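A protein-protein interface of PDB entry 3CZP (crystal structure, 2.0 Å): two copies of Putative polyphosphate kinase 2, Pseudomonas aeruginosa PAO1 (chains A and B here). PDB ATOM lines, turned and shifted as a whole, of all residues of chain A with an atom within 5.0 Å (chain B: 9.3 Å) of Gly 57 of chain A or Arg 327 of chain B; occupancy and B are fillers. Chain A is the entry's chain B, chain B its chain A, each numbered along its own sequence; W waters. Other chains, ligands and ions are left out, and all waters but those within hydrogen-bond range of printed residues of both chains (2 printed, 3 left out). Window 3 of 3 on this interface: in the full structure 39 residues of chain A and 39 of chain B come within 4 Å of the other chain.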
ATOM      1  N   GLY A  55      21.079  24.004   3.218  1.00  0.00           N
ATOM      2  CA  GLY A  55      20.629  25.155   2.451  1.00  0.00           C
ATOM      3  C   GLY A  55      20.893  25.126   0.956  1.00  0.00           C
ATOM      4  O   GLY A  55      20.822  26.172   0.317  1.00  0.00           O
ATOM      5  N   LYS A  56      21.196  23.951   0.402  1.00  0.00           N
ATOM      6  CA  LYS A  56      21.440  23.799  -1.049  1.00  0.00           C
ATOM      7  C   LYS A  56      20.298  24.357  -1.894  1.00  0.00           C
ATOM      8  O   LYS A  56      20.504  25.291  -2.636  1.00  0.00           O
ATOM      9  CB  LYS A  56      21.720  22.329  -1.437  1.00  0.00           C
ATOM     10  CG  LYS A  56      23.033  21.772  -0.872  1.00  0.00           C
ATOM     11  CD  LYS A  56      23.330  20.282  -1.252  1.00  0.00           C
ATOM     12  CE  LYS A  56      22.270  19.268  -0.752  1.00  0.00           C
ATOM     13  NZ  LYS A  56      22.586  17.860  -1.156  1.00  0.00           N
ATOM     14  N   GLY A  57      19.101  23.798  -1.748  1.00  0.00           N
ATOM     15  CA  GLY A  57      17.982  24.179  -2.583  1.00  0.00           C
ATOM     16  C   GLY A  57      17.501  25.589  -2.310  1.00  0.00           C
ATOM     17  O   GLY A  57      17.117  26.308  -3.239  1.00  0.00           O
ATOM     18  N   GLU A  58      17.523  25.983  -1.029  1.00  0.00           N
ATOM     19  CA  GLU A  58      17.041  27.310  -0.607  1.00  0.00           C
ATOM     20  C   GLU A  58      17.945  28.376  -1.195  1.00  0.00           C
ATOM     21  O   GLU A  58      17.487  29.403  -1.658  1.00  0.00           O
ATOM     22  CB  GLU A  58      17.013  27.423   0.937  1.00  0.00           C
ATOM     23  CG  GLU A  58      15.950  26.523   1.619  1.00  0.00           C
ATOM     24  CD  GLU A  58      16.405  25.061   1.864  1.00  0.00           C
ATOM     25  OE1 GLU A  58      17.429  24.595   1.276  1.00  0.00           O
ATOM     26  OE2 GLU A  58      15.705  24.368   2.656  1.00  0.00           O
ATOM     27  N   THR A  59      19.250  28.107  -1.178  1.00  0.00           N
ATOM     28  CA  THR A  59      20.219  29.052  -1.708  1.00  0.00           C
ATOM     29  C   THR A  59      20.090  29.175  -3.226  1.00  0.00           C
ATOM     30  O   THR A  59      20.083  30.290  -3.739  1.00  0.00           O
ATOM     31  CB  THR A  59      21.667  28.719  -1.297  1.00  0.00           C
ATOM     32  OG1 THR A  59      21.740  28.442   0.115  1.00  0.00           O
ATOM     33  CG2 THR A  59      22.603  29.893  -1.659  1.00  0.00           C
ATOM     34  N   VAL A  60      19.926  28.064  -3.945  1.00  0.00           N
ATOM     35  CA  VAL A  60      19.729  28.165  -5.403  1.00  0.00           C
ATOM     36  C   VAL A  60      18.442  28.922  -5.788  1.00  0.00           C
ATOM     37  O   VAL A  60      18.458  29.776  -6.711  1.00  0.00           O
ATOM     38  CB  VAL A  60      19.910  26.770  -6.113  1.00  0.00           C
ATOM     39  CG1 VAL A  60      19.472  26.755  -7.597  1.00  0.00           C
ATOM     40  CG2 VAL A  60      21.349  26.369  -6.029  1.00  0.00           C
ATOM     41  N   LYS A  61      17.353  28.667  -5.058  1.00  0.00           N
ATOM     42  CA  LYS A  61      16.118  29.458  -5.205  1.00  0.00           C
ATOM     43  C   LYS A  61      16.378  30.943  -5.030  1.00  0.00           C
ATOM     44  O   LYS A  61      15.967  31.740  -5.857  1.00  0.00           O
ATOM     45  CB  LYS A  61      15.010  29.005  -4.217  1.00  0.00           C
ATOM     46  CG  LYS A  61      13.603  29.572  -4.568  1.00  0.00           C
ATOM     47  CD  LYS A  61      12.536  29.038  -3.680  1.00  0.00           C
ATOM     48  CE  LYS A  61      11.261  29.866  -3.804  1.00  0.00           C
ATOM     49  NZ  LYS A  61      10.150  29.082  -3.248  1.00  0.00           N
ATOM     50  N   VAL A  74      18.653  25.267 -14.256  1.00  0.00           N
ATOM     51  CA  VAL A  74      18.987  24.470 -13.083  1.00  0.00           C
ATOM     52  C   VAL A  74      18.668  23.041 -13.411  1.00  0.00           C
ATOM     53  O   VAL A  74      17.538  22.752 -13.798  1.00  0.00           O
ATOM     54  CB  VAL A  74      18.256  24.928 -11.793  1.00  0.00           C
ATOM     55  CG1 VAL A  74      18.666  24.064 -10.600  1.00  0.00           C
ATOM     56  CG2 VAL A  74      18.611  26.331 -11.438  1.00  0.00           C
ATOM     57  N   SER A  76      18.926  18.820 -12.211  1.00  0.00           N
ATOM     58  CA  SER A  76      19.367  17.692 -11.402  1.00  0.00           C
ATOM     59  C   SER A  76      19.530  16.466 -12.258  1.00  0.00           C
ATOM     60  O   SER A  76      18.859  16.313 -13.272  1.00  0.00           O
ATOM     61  CB  SER A  76      18.438  17.397 -10.259  1.00  0.00           C
ATOM     62  OG  SER A  76      19.106  16.397  -9.517  1.00  0.00           O
ATOM     63  N   PHE A 107      22.607  20.295  -9.643  1.00  0.00           N
ATOM     64  CA  PHE A 107      22.461  19.488  -8.430  1.00  0.00           C
ATOM     65  C   PHE A 107      22.768  18.103  -8.941  1.00  0.00           C
ATOM     66  O   PHE A 107      22.762  17.866 -10.135  1.00  0.00           O
ATOM     67  CB  PHE A 107      21.035  19.500  -7.866  1.00  0.00           C
ATOM     68  CG  PHE A 107      20.571  20.829  -7.303  1.00  0.00           C
ATOM     69  CD1 PHE A 107      20.568  21.044  -5.926  1.00  0.00           C
ATOM     70  CD2 PHE A 107      20.088  21.837  -8.134  1.00  0.00           C
ATOM     71  CE1 PHE A 107      20.132  22.240  -5.367  1.00  0.00           C
ATOM     72  CE2 PHE A 107      19.654  23.035  -7.593  1.00  0.00           C
ATOM     73  CZ  PHE A 107      19.656  23.232  -6.179  1.00  0.00           C
ATOM     74  N   ILE B 291       0.984  22.898  -8.491  1.00  0.00           N
ATOM     75  CA  ILE B 291       2.117  22.219  -9.131  1.00  0.00           C
ATOM     76  C   ILE B 291       2.513  20.942  -8.383  1.00  0.00           C
ATOM     77  O   ILE B 291       2.915  19.953  -9.005  1.00  0.00           O
ATOM     78  CB  ILE B 291       3.337  23.148  -9.249  1.00  0.00           C
ATOM     79  CG1 ILE B 291       3.054  24.278 -10.224  1.00  0.00           C
ATOM     80  CG2 ILE B 291       4.557  22.390  -9.708  1.00  0.00           C
ATOM     81  CD1 ILE B 291       2.858  23.856 -11.564  1.00  0.00           C
ATOM     82  N   THR B 321       8.089  32.675 -11.028  1.00  0.00           N
ATOM     83  CA  THR B 321       9.210  31.789 -10.658  1.00  0.00           C
ATOM     84  C   THR B 321       9.443  31.841  -9.151  1.00  0.00           C
ATOM     85  O   THR B 321       9.827  30.835  -8.575  1.00  0.00           O
ATOM     86  CB  THR B 321      10.566  32.076 -11.462  1.00  0.00           C
ATOM     87  OG1 THR B 321      11.016  33.399 -11.244  1.00  0.00           O
ATOM     88  CG2 THR B 321      10.390  31.891 -12.961  1.00  0.00           C
ATOM     89  N   LEU B 324       8.068  29.141  -7.017  1.00  0.00           N
ATOM     90  CA  LEU B 324       8.531  27.760  -7.143  1.00  0.00           C
ATOM     91  C   LEU B 324      10.036  27.551  -6.958  1.00  0.00           C
ATOM     92  O   LEU B 324      10.810  28.494  -6.860  1.00  0.00           O
ATOM     93  CB  LEU B 324       8.128  27.217  -8.515  1.00  0.00           C
ATOM     94  CG  LEU B 324       6.696  27.386  -9.012  1.00  0.00           C
ATOM     95  CD1 LEU B 324       6.692  27.281 -10.528  1.00  0.00           C
ATOM     96  CD2 LEU B 324       5.697  26.437  -8.372  1.00  0.00           C
ATOM     97  N   ASP B 325      10.439  26.289  -6.909  1.00  0.00           N
ATOM     98  CA  ASP B 325      11.853  25.924  -6.893  1.00  0.00           C
ATOM     99  C   ASP B 325      12.351  25.963  -8.359  1.00  0.00           C
ATOM    100  O   ASP B 325      11.591  25.681  -9.274  1.00  0.00           O
ATOM    101  CB  ASP B 325      12.012  24.541  -6.240  1.00  0.00           C
ATOM    102  CG  ASP B 325      13.461  24.101  -6.124  1.00  0.00           C
ATOM    103  OD1 ASP B 325      14.111  23.850  -7.165  1.00  0.00           O
ATOM    104  OD2 ASP B 325      13.947  23.970  -4.986  1.00  0.00           O
ATOM    105  N   PRO B 326      13.602  26.385  -8.598  1.00  0.00           N
ATOM    106  CA  PRO B 326      14.045  26.411 -10.004  1.00  0.00           C
ATOM    107  C   PRO B 326      14.127  25.073 -10.720  1.00  0.00           C
ATOM    108  O   PRO B 326      14.127  25.047 -11.913  1.00  0.00           O
ATOM    109  CB  PRO B 326      15.425  27.090  -9.933  1.00  0.00           C
ATOM    110  CG  PRO B 326      15.448  27.743  -8.658  1.00  0.00           C
ATOM    111  CD  PRO B 326      14.632  26.937  -7.715  1.00  0.00           C
ATOM    112  N   ARG B 327      14.228  23.968 -10.009  1.00  0.00           N
ATOM    113  CA  ARG B 327      14.136  22.635 -10.623  1.00  0.00           C
ATOM    114  C   ARG B 327      12.757  22.345 -11.178  1.00  0.00           C
ATOM    115  O   ARG B 327      12.596  21.386 -11.907  1.00  0.00           O
ATOM    116  CB  ARG B 327      14.529  21.541  -9.609  1.00  0.00           C
ATOM    117  CG  ARG B 327      16.022  21.606  -9.246  1.00  0.00           C
ATOM    118  CD  ARG B 327      16.354  20.810  -8.019  1.00  0.00           C
ATOM    119  NE  ARG B 327      15.885  21.490  -6.818  1.00  0.00           N
ATOM    120  CZ  ARG B 327      16.210  21.132  -5.578  1.00  0.00           C
ATOM    121  NH1 ARG B 327      17.025  20.100  -5.375  1.00  0.00           N
ATOM    122  NH2 ARG B 327      15.733  21.812  -4.532  1.00  0.00           N
ATOM    123  N   GLN B 328      11.780  23.194 -10.880  1.00  0.00           N
ATOM    124  CA  GLN B 328      10.406  22.982 -11.343  1.00  0.00           C
ATOM    125  C   GLN B 328      10.026  23.653 -12.685  1.00  0.00           C
ATOM    126  O   GLN B 328       8.908  23.456 -13.181  1.00  0.00           O
ATOM    127  CB  GLN B 328       9.450  23.435 -10.245  1.00  0.00           C
ATOM    128  CG  GLN B 328       9.472  22.561  -8.992  1.00  0.00           C
ATOM    129  CD  GLN B 328       8.519  23.097  -7.914  1.00  0.00           C
ATOM    130  OE1 GLN B 328       8.776  24.132  -7.290  1.00  0.00           O
ATOM    131  NE2 GLN B 328       7.434  22.384  -7.680  1.00  0.00           N
ATOM    132  N   TYR B 329      10.911  24.474 -13.248  1.00  0.00           N
ATOM    133  CA  TYR B 329      10.567  25.271 -14.397  1.00  0.00           C
ATOM    134  C   TYR B 329      11.789  25.430 -15.277  1.00  0.00           C
ATOM    135  O   TYR B 329      12.913  25.097 -14.868  1.00  0.00           O
ATOM    136  CB  TYR B 329       9.909  26.620 -14.014  1.00  0.00           C
ATOM    137  CG  TYR B 329      10.791  27.509 -13.169  1.00  0.00           C
ATOM    138  CD1 TYR B 329      11.894  28.153 -13.735  1.00  0.00           C
ATOM    139  CD2 TYR B 329      10.546  27.698 -11.801  1.00  0.00           C
ATOM    140  CE1 TYR B 329      12.704  28.948 -13.001  1.00  0.00           C
ATOM    141  CE2 TYR B 329      11.387  28.513 -11.037  1.00  0.00           C
ATOM    142  CZ  TYR B 329      12.445  29.135 -11.641  1.00  0.00           C
ATOM    143  OH  TYR B 329      13.311  29.913 -10.944  1.00  0.00           O
ATOM    144  N   HIS B 330      11.526  25.880 -16.513  1.00  0.00           N
ATOM    145  CA  HIS B 330      12.539  26.093 -17.550  1.00  0.00           C
ATOM    146  C   HIS B 330      12.078  27.327 -18.302  1.00  0.00           C
ATOM    147  O   HIS B 330      10.982  27.314 -18.842  1.00  0.00           O
ATOM    148  CB  HIS B 330      12.589  24.878 -18.464  1.00  0.00           C
ATOM    149  CG  HIS B 330      13.504  25.034 -19.649  1.00  0.00           C
ATOM    150  ND1 HIS B 330      14.796  25.523 -19.542  1.00  0.00           N
ATOM    151  CD2 HIS B 330      13.334  24.705 -20.952  1.00  0.00           C
ATOM    152  CE1 HIS B 330      15.374  25.497 -20.729  1.00  0.00           C
ATOM    153  NE2 HIS B 330      14.508  25.012 -21.608  1.00  0.00           N
ATOM    154  N   ARG B 358       4.900  16.797 -16.230  1.00  0.00           N
ATOM    155  CA  ARG B 358       5.229  17.345 -14.929  1.00  0.00           C
ATOM    156  C   ARG B 358       6.154  18.539 -14.987  1.00  0.00           C
ATOM    157  O   ARG B 358       6.513  19.021 -13.967  1.00  0.00           O
ATOM    158  CB  ARG B 358       5.811  16.281 -14.010  1.00  0.00           C
ATOM    159  CG  ARG B 358       5.403  16.486 -12.576  1.00  0.00           C
ATOM    160  CD  ARG B 358       5.621  15.204 -11.857  1.00  0.00           C
ATOM    161  NE  ARG B 358       5.758  15.433 -10.428  1.00  0.00           N
ATOM    162  CZ  ARG B 358       6.738  14.929  -9.683  1.00  0.00           C
ATOM    163  NH1 ARG B 358       7.685  14.151 -10.236  1.00  0.00           N
ATOM    164  NH2 ARG B 358       6.770  15.191  -8.379  1.00  0.00           N
ATOM    165  N   GLN B 359       6.502  19.036 -16.171  1.00  0.00           N
ATOM    166  CA  GLN B 359       7.406  20.176 -16.286  1.00  0.00           C
ATOM    167  C   GLN B 359       6.610  21.438 -16.628  1.00  0.00           C
ATOM    168  O   GLN B 359       5.428  21.381 -17.016  1.00  0.00           O
ATOM    169  CB  GLN B 359       8.516  19.954 -17.352  1.00  0.00           C
ATOM    170  CG  GLN B 359       9.444  18.763 -17.131  1.00  0.00           C
ATOM    171  CD  GLN B 359      10.571  18.604 -18.225  1.00  0.00           C
ATOM    172  OE1 GLN B 359      10.497  19.149 -19.337  1.00  0.00           O
ATOM    173  NE2 GLN B 359      11.626  17.878 -17.867  1.00  0.00           N
ATOM    174  N   PHE B 360       7.287  22.579 -16.506  1.00  0.00           N
ATOM    175  CA  PHE B 360       6.680  23.909 -16.699  1.00  0.00           C
ATOM    176  C   PHE B 360       7.652  24.738 -17.510  1.00  0.00           C
ATOM    177  O   PHE B 360       8.749  24.945 -17.088  1.00  0.00           O
ATOM    178  CB  PHE B 360       6.433  24.538 -15.310  1.00  0.00           C
ATOM    179  CG  PHE B 360       5.824  25.942 -15.308  1.00  0.00           C
ATOM    180  CD1 PHE B 360       5.301  26.552 -16.472  1.00  0.00           C
ATOM    181  CD2 PHE B 360       5.789  26.641 -14.125  1.00  0.00           C
ATOM    182  CE1 PHE B 360       4.754  27.829 -16.427  1.00  0.00           C
ATOM    183  CE2 PHE B 360       5.264  27.933 -14.062  1.00  0.00           C
ATOM    184  CZ  PHE B 360       4.745  28.534 -15.205  1.00  0.00           C
HETATM  185  O   HOH W   1      15.609  26.616 -13.931  1.00  0.00           O
HETATM  186  O   HOH W   2      16.764  25.276  -5.886  1.00  0.00           O
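No position is printed for both chains.
Printed residues of chain A that touch a printed residue of chain B: Gly 57, Lys 61, Val 74 and Phe 107. Printed residues of chain B that touch a printed residue of chain A: Leu 324, Pro 326 and Arg 327.
Among the printed residues, pairs that only touch across the chains: Lys 61 of chain A with Leu 324 of chain B, Val 74 of chain A with Pro 326 of chain B, Phe 107 of chain A with Arg 327 of chain B, Gly 57 of chain A with Arg 327 of chain B, Lys 61 of chain A with Pro 326 of chain B and Val 74 of chain A with Arg 327 of chain B.
The guanidinium group (NH2) of Arg 327 of chain B is in salt-bridge range of the side-chain carboxylate (OD2) of Asp 325 of chain B, 2.8 Å away.
Water W2 bridges the backbone carbonyl oxygen of Gly 57 of chain A and the side-chain carboxylate of Asp 325 of chain B. Water W1 lies within hydrogen-bond range of the backbone carbonyl oxygen (O) of Pro 326 of chain B (3.0 Å), the backbone carbonyl oxygen (O) of Tyr 329 of chain B (3.2 Å) and the backbone NH (N) of Val 74 of chain A (3.3 Å).
Gly 57 of chain A touches one residue of chain B. No residue of chain B comes within 4 Å of Val 60 of chain A. Printed residues of chain B within 4 Å of Val 74 of chain A: Pro 326 (3.6 Å) and Arg 327 (3.9 Å). Of the printed residues of chain A, Pro 326 of chain B touches Lys 61 and Val 74. Arg 327 of chain B touches just these residues of chain A: Gly 57 (3.8 Å), Val 74 (3.9 Å) and Phe 107 (3.7 Å). The nearest printed residue of chain B that does not touch Val 74 of chain A is Tyr 329 of chain B (5.3 Å).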
